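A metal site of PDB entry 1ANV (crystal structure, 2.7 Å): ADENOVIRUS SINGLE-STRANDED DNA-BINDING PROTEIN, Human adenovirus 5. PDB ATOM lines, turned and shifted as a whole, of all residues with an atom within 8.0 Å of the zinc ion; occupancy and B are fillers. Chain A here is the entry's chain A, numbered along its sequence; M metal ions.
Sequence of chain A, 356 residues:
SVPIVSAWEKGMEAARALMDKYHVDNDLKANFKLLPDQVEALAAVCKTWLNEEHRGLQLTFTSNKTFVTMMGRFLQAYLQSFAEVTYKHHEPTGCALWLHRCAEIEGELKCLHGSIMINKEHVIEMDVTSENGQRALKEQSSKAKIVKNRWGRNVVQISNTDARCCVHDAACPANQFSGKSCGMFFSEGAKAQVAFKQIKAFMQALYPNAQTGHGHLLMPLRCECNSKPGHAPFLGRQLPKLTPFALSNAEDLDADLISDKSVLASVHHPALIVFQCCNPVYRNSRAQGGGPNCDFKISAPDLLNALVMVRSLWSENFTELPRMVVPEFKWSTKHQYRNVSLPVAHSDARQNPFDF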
ATOM      1  N   ARG A 222     -10.365  24.505  -1.530  1.00  0.00           N
ATOM      2  CA  ARG A 222     -11.161  25.708  -1.418  1.00  0.00           C
ATOM      3  C   ARG A 222     -11.360  26.427  -2.715  1.00  0.00           C
ATOM      4  O   ARG A 222     -10.517  26.381  -3.609  1.00  0.00           O
ATOM      5  CB  ARG A 222     -10.649  26.688  -0.352  1.00  0.00           C
ATOM      6  CG  ARG A 222      -9.165  26.976  -0.440  1.00  0.00           C
ATOM      7  CD  ARG A 222      -8.635  27.688   0.790  1.00  0.00           C
ATOM      8  NE  ARG A 222      -7.441  28.489   0.471  1.00  0.00           N
ATOM      9  CZ  ARG A 222      -6.248  28.314   1.021  1.00  0.00           C
ATOM     10  NH1 ARG A 222      -6.028  27.373   1.937  1.00  0.00           N
ATOM     11  NH2 ARG A 222      -5.249  29.093   0.644  1.00  0.00           N
ATOM     12  N   CYS A 223     -12.501  27.067  -2.794  1.00  0.00           N
ATOM     13  CA  CYS A 223     -12.843  27.822  -3.957  1.00  0.00           C
ATOM     14  C   CYS A 223     -12.931  29.272  -3.562  1.00  0.00           C
ATOM     15  O   CYS A 223     -12.417  29.710  -2.534  1.00  0.00           O
ATOM     16  CB  CYS A 223     -14.177  27.395  -4.579  1.00  0.00           C
ATOM     17  SG  CYS A 223     -15.564  27.664  -3.487  1.00  0.00           S
ATOM     18  N   GLU A 224     -13.610  30.011  -4.402  1.00  0.00           N
ATOM     19  CA  GLU A 224     -13.772  31.408  -4.106  1.00  0.00           C
ATOM     20  C   GLU A 224     -14.512  31.556  -2.790  1.00  0.00           C
ATOM     21  O   GLU A 224     -14.207  32.407  -1.978  1.00  0.00           O
ATOM     22  CB  GLU A 224     -14.510  32.100  -5.276  1.00  0.00           C
ATOM     23  CG  GLU A 224     -14.576  33.631  -5.196  1.00  0.00           C
ATOM     24  CD  GLU A 224     -15.641  34.159  -6.104  1.00  0.00           C
ATOM     25  OE1 GLU A 224     -15.306  34.109  -7.372  1.00  0.00           O
ATOM     26  OE2 GLU A 224     -16.712  34.582  -5.700  1.00  0.00           O
ATOM     27  N   CYS A 225     -15.485  30.691  -2.549  1.00  0.00           N
ATOM     28  CA  CYS A 225     -16.268  30.758  -1.342  1.00  0.00           C
ATOM     29  C   CYS A 225     -15.536  30.617  -0.025  1.00  0.00           C
ATOM     30  O   CYS A 225     -15.763  31.392   0.901  1.00  0.00           O
ATOM     31  CB  CYS A 225     -17.481  29.873  -1.440  1.00  0.00           C
ATOM     32  SG  CYS A 225     -18.297  30.273  -2.995  1.00  0.00           S
ATOM     33  N   ASN A 226     -14.690  29.632   0.079  1.00  0.00           N
ATOM     34  CA  ASN A 226     -13.964  29.432   1.313  1.00  0.00           C
ATOM     35  C   ASN A 226     -12.529  29.834   1.127  1.00  0.00           C
ATOM     36  O   ASN A 226     -11.617  29.287   1.719  1.00  0.00           O
ATOM     37  CB  ASN A 226     -14.079  27.978   1.797  1.00  0.00           C
ATOM     38  CG  ASN A 226     -13.771  27.019   0.678  1.00  0.00           C
ATOM     39  OD1 ASN A 226     -13.646  27.452  -0.485  1.00  0.00           O
ATOM     40  ND2 ASN A 226     -13.620  25.755   1.031  1.00  0.00           N
ATOM     41  N   SER A 227     -12.343  30.806   0.254  1.00  0.00           N
ATOM     42  CA  SER A 227     -11.010  31.283  -0.035  1.00  0.00           C
ATOM     43  C   SER A 227     -10.256  31.757   1.207  1.00  0.00           C
ATOM     44  O   SER A 227      -9.057  31.568   1.346  1.00  0.00           O
ATOM     45  CB  SER A 227     -11.075  32.452  -0.994  1.00  0.00           C
ATOM     46  OG  SER A 227     -11.719  33.518  -0.322  1.00  0.00           O
ATOM     47  N   PHE A 234     -20.727  28.602   5.716  1.00  0.00           N
ATOM     48  CA  PHE A 234     -21.826  28.383   4.798  1.00  0.00           C
ATOM     49  C   PHE A 234     -22.226  26.924   4.753  1.00  0.00           C
ATOM     50  O   PHE A 234     -21.379  26.034   4.885  1.00  0.00           O
ATOM     51  CB  PHE A 234     -21.576  28.979   3.393  1.00  0.00           C
ATOM     52  CG  PHE A 234     -20.375  28.389   2.696  1.00  0.00           C
ATOM     53  CD1 PHE A 234     -20.475  27.204   1.983  1.00  0.00           C
ATOM     54  CD2 PHE A 234     -19.126  29.023   2.764  1.00  0.00           C
ATOM     55  CE1 PHE A 234     -19.384  26.648   1.320  1.00  0.00           C
ATOM     56  CE2 PHE A 234     -18.019  28.478   2.130  1.00  0.00           C
ATOM     57  CZ  PHE A 234     -18.146  27.289   1.397  1.00  0.00           C
ATOM     58  N   ARG A 237     -21.818  21.618   0.825  1.00  0.00           N
ATOM     59  CA  ARG A 237     -20.515  21.012   0.635  1.00  0.00           C
ATOM     60  C   ARG A 237     -19.414  21.991   1.063  1.00  0.00           C
ATOM     61  O   ARG A 237     -19.385  23.161   0.699  1.00  0.00           O
ATOM     62  CB  ARG A 237     -20.324  20.476  -0.780  1.00  0.00           C
ATOM     63  CG  ARG A 237     -18.878  20.071  -1.057  1.00  0.00           C
ATOM     64  CD  ARG A 237     -18.675  19.399  -2.401  1.00  0.00           C
ATOM     65  NE  ARG A 237     -19.685  18.371  -2.668  1.00  0.00           N
ATOM     66  CZ  ARG A 237     -20.822  18.611  -3.302  1.00  0.00           C
ATOM     67  NH1 ARG A 237     -21.143  19.810  -3.741  1.00  0.00           N
ATOM     68  NH2 ARG A 237     -21.671  17.611  -3.497  1.00  0.00           N
ATOM     69  N   LEU A 239     -16.203  21.628   0.381  1.00  0.00           N
ATOM     70  CA  LEU A 239     -15.060  21.474  -0.518  1.00  0.00           C
ATOM     71  C   LEU A 239     -15.538  21.629  -1.935  1.00  0.00           C
ATOM     72  O   LEU A 239     -16.730  21.480  -2.233  1.00  0.00           O
ATOM     73  CB  LEU A 239     -14.462  20.054  -0.445  1.00  0.00           C
ATOM     74  CG  LEU A 239     -13.370  19.833   0.591  1.00  0.00           C
ATOM     75  CD1 LEU A 239     -12.620  18.531   0.288  1.00  0.00           C
ATOM     76  CD2 LEU A 239     -12.377  20.991   0.591  1.00  0.00           C
ATOM     77  N   PRO A 240     -14.626  21.904  -2.825  1.00  0.00           N
ATOM     78  CA  PRO A 240     -15.047  22.052  -4.185  1.00  0.00           C
ATOM     79  C   PRO A 240     -15.582  20.731  -4.689  1.00  0.00           C
ATOM     80  O   PRO A 240     -15.078  19.671  -4.311  1.00  0.00           O
ATOM     81  CB  PRO A 240     -13.830  22.552  -4.971  1.00  0.00           C
ATOM     82  CG  PRO A 240     -12.821  23.018  -3.931  1.00  0.00           C
ATOM     83  CD  PRO A 240     -13.251  22.406  -2.600  1.00  0.00           C
ATOM     84  N   GLN A 276     -15.507  22.250  -9.326  1.00  0.00           N
ATOM     85  CA  GLN A 276     -16.222  23.506  -9.402  1.00  0.00           C
ATOM     86  C   GLN A 276     -16.346  24.123  -8.021  1.00  0.00           C
ATOM     87  O   GLN A 276     -15.535  23.864  -7.158  1.00  0.00           O
ATOM     88  CB  GLN A 276     -17.611  23.342  -9.995  1.00  0.00           C
ATOM     89  CG  GLN A 276     -17.546  22.827 -11.438  1.00  0.00           C
ATOM     90  CD  GLN A 276     -18.642  21.836 -11.718  1.00  0.00           C
ATOM     91  OE1 GLN A 276     -18.843  20.875 -10.953  1.00  0.00           O
ATOM     92  NE2 GLN A 276     -19.368  22.088 -12.808  1.00  0.00           N
ATOM     93  N   CYS A 277     -17.373  24.950  -7.822  1.00  0.00           N
ATOM     94  CA  CYS A 277     -17.576  25.576  -6.534  1.00  0.00           C
ATOM     95  C   CYS A 277     -17.910  24.521  -5.510  1.00  0.00           C
ATOM     96  O   CYS A 277     -18.156  23.378  -5.863  1.00  0.00           O
ATOM     97  CB  CYS A 277     -18.762  26.567  -6.599  1.00  0.00           C
ATOM     98  SG  CYS A 277     -18.951  27.579  -5.100  1.00  0.00           S
ATOM     99  N   CYS A 278     -17.934  24.919  -4.240  1.00  0.00           N
ATOM    100  CA  CYS A 278     -18.275  23.989  -3.182  1.00  0.00           C
ATOM    101  C   CYS A 278     -19.684  23.506  -3.431  1.00  0.00           C
ATOM    102  O   CYS A 278     -20.026  22.329  -3.272  1.00  0.00           O
ATOM    103  CB  CYS A 278     -18.168  24.644  -1.803  1.00  0.00           C
ATOM    104  SG  CYS A 278     -16.459  24.766  -1.265  1.00  0.00           S
ATOM    105  N   ASN A 279     -20.484  24.462  -3.864  1.00  0.00           N
ATOM    106  CA  ASN A 279     -21.854  24.228  -4.182  1.00  0.00           C
ATOM    107  C   ASN A 279     -22.238  25.024  -5.410  1.00  0.00           C
ATOM    108  O   ASN A 279     -22.425  26.236  -5.336  1.00  0.00           O
ATOM    109  CB  ASN A 279     -22.746  24.616  -2.998  1.00  0.00           C
ATOM    110  CG  ASN A 279     -22.229  24.080  -1.670  1.00  0.00           C
ATOM    111  OD1 ASN A 279     -22.285  22.870  -1.379  1.00  0.00           O
ATOM    112  ND2 ASN A 279     -21.737  24.985  -0.846  1.00  0.00           N
ATOM    113  N   PRO A 280     -22.346  24.337  -6.541  1.00  0.00           N
ATOM    114  CA  PRO A 280     -22.719  24.992  -7.784  1.00  0.00           C
ATOM    115  C   PRO A 280     -24.222  24.871  -8.019  1.00  0.00           C
ATOM    116  O   PRO A 280     -24.861  25.734  -8.640  1.00  0.00           O
ATOM    117  CB  PRO A 280     -21.938  24.260  -8.893  1.00  0.00           C
ATOM    118  CG  PRO A 280     -21.429  22.955  -8.284  1.00  0.00           C
ATOM    119  CD  PRO A 280     -21.661  23.050  -6.782  1.00  0.00           C
ATOM    120  N   PRO A 292     -23.750  31.128  -0.720  1.00  0.00           N
ATOM    121  CA  PRO A 292     -22.773  31.608  -1.673  1.00  0.00           C
ATOM    122  C   PRO A 292     -22.541  30.609  -2.792  1.00  0.00           C
ATOM    123  O   PRO A 292     -22.791  29.401  -2.638  1.00  0.00           O
ATOM    124  CB  PRO A 292     -21.482  31.856  -0.900  1.00  0.00           C
ATOM    125  CG  PRO A 292     -21.667  31.224   0.480  1.00  0.00           C
ATOM    126  CD  PRO A 292     -23.094  30.720   0.553  1.00  0.00           C
ATOM    127  N   ASN A 293     -22.057  31.126  -3.910  1.00  0.00           N
ATOM    128  CA  ASN A 293     -21.743  30.368  -5.109  1.00  0.00           C
ATOM    129  C   ASN A 293     -20.719  31.123  -5.938  1.00  0.00           C
ATOM    130  O   ASN A 293     -20.854  32.319  -6.166  1.00  0.00           O
ATOM    131  CB  ASN A 293     -22.972  30.067  -5.988  1.00  0.00           C
ATOM    132  CG  ASN A 293     -22.567  29.754  -7.432  1.00  0.00           C
ATOM    133  OD1 ASN A 293     -22.726  30.578  -8.344  1.00  0.00           O
ATOM    134  ND2 ASN A 293     -22.016  28.554  -7.642  1.00  0.00           N
ATOM    135  N   CYS A 294     -19.706  30.421  -6.417  1.00  0.00           N
ATOM    136  CA  CYS A 294     -18.732  31.092  -7.240  1.00  0.00           C
ATOM    137  C   CYS A 294     -18.627  30.398  -8.573  1.00  0.00           C
ATOM    138  O   CYS A 294     -19.221  29.333  -8.740  1.00  0.00           O
ATOM    139  CB  CYS A 294     -17.366  31.298  -6.577  1.00  0.00           C
ATOM    140  SG  CYS A 294     -16.481  29.755  -6.247  1.00  0.00           S
ATOM    141  N   ASP A 295     -17.892  31.020  -9.497  1.00  0.00           N
ATOM    142  CA  ASP A 295     -17.714  30.459 -10.826  1.00  0.00           C
ATOM    143  C   ASP A 295     -16.374  29.733 -10.998  1.00  0.00           C
ATOM    144  O   ASP A 295     -15.781  29.700 -12.095  1.00  0.00           O
ATOM    145  CB  ASP A 295     -18.054  31.490 -11.931  1.00  0.00           C
ATOM    146  CG  ASP A 295     -19.318  31.170 -12.675  1.00  0.00           C
ATOM    147  OD1 ASP A 295     -20.427  31.563 -12.344  1.00  0.00           O
ATOM    148  OD2 ASP A 295     -19.122  30.411 -13.723  1.00  0.00           O
ATOM    149  N   PHE A 296     -15.921  29.121  -9.903  1.00  0.00           N
ATOM    150  CA  PHE A 296     -14.687  28.347  -9.870  1.00  0.00           C
ATOM    151  C   PHE A 296     -14.793  27.085 -10.715  1.00  0.00           C
ATOM    152  O   PHE A 296     -15.705  26.270 -10.540  1.00  0.00           O
ATOM    153  CB  PHE A 296     -14.358  27.959  -8.432  1.00  0.00           C
ATOM    154  CG  PHE A 296     -13.018  27.310  -8.195  1.00  0.00           C
ATOM    155  CD1 PHE A 296     -12.881  25.929  -8.256  1.00  0.00           C
ATOM    156  CD2 PHE A 296     -11.912  28.077  -7.826  1.00  0.00           C
ATOM    157  CE1 PHE A 296     -11.662  25.331  -7.972  1.00  0.00           C
ATOM    158  CE2 PHE A 296     -10.670  27.490  -7.544  1.00  0.00           C
ATOM    159  CZ  PHE A 296     -10.550  26.103  -7.622  1.00  0.00           C
HETATM  160 ZN    ZN M   1     -17.358  28.817  -4.346  1.00  0.00          ZN
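Merely in contact with the zinc ion: Glu 224 (3.9 Å) and Cys 278 (3.9 Å).
Six residues have an atom within 4 Å of the zinc ion: Cys 223, Glu 224, Cys 225, Cys 277, Cys 278 and Cys 294.
The nearest printed residue that does not touch the zinc ion is Asn 293 (4.4 Å).
The zinc ion is bound by the side-chain sulfur of Cys 277 (2.2 Å), the side-chain sulfur of Cys 225 (2.2 Å), the side-chain sulfur of Cys 294 (2.3 Å) and the side-chain sulfur of Cys 223 (2.3 Å).
The zinc ion has four donor atoms within binding distance.
N of Phe 296 sits close to SG of Cys 294 (3.8 Å).
SG of Cys 294 lies close to N of Glu 224.
The side-chain sulfur (SG) of Cys 277 lies close to the backbone NH (N) of Asn 279, at 3.7 Å.
The side-chain sulfur (SG) of Cys 278 sits at hydrogen-bond distance from the side-chain amide nitrogen (ND2) of Asn 226 (3.8 Å).
O of Cys 278 lies within hydrogen-bond range of NH1 of Arg 237.
The side-chain sulfur (SG) of Cys 223 sits close to the backbone NH (N) of Cys 278 (3.7 Å).
The backbone carbonyl oxygen (O) of Glu 224 is in hydrogen-bond range of the side-chain hydroxyl (OG) of Ser 227 (3.2 Å).
N of Cys 277 is in hydrogen-bond range of O of Phe 296.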
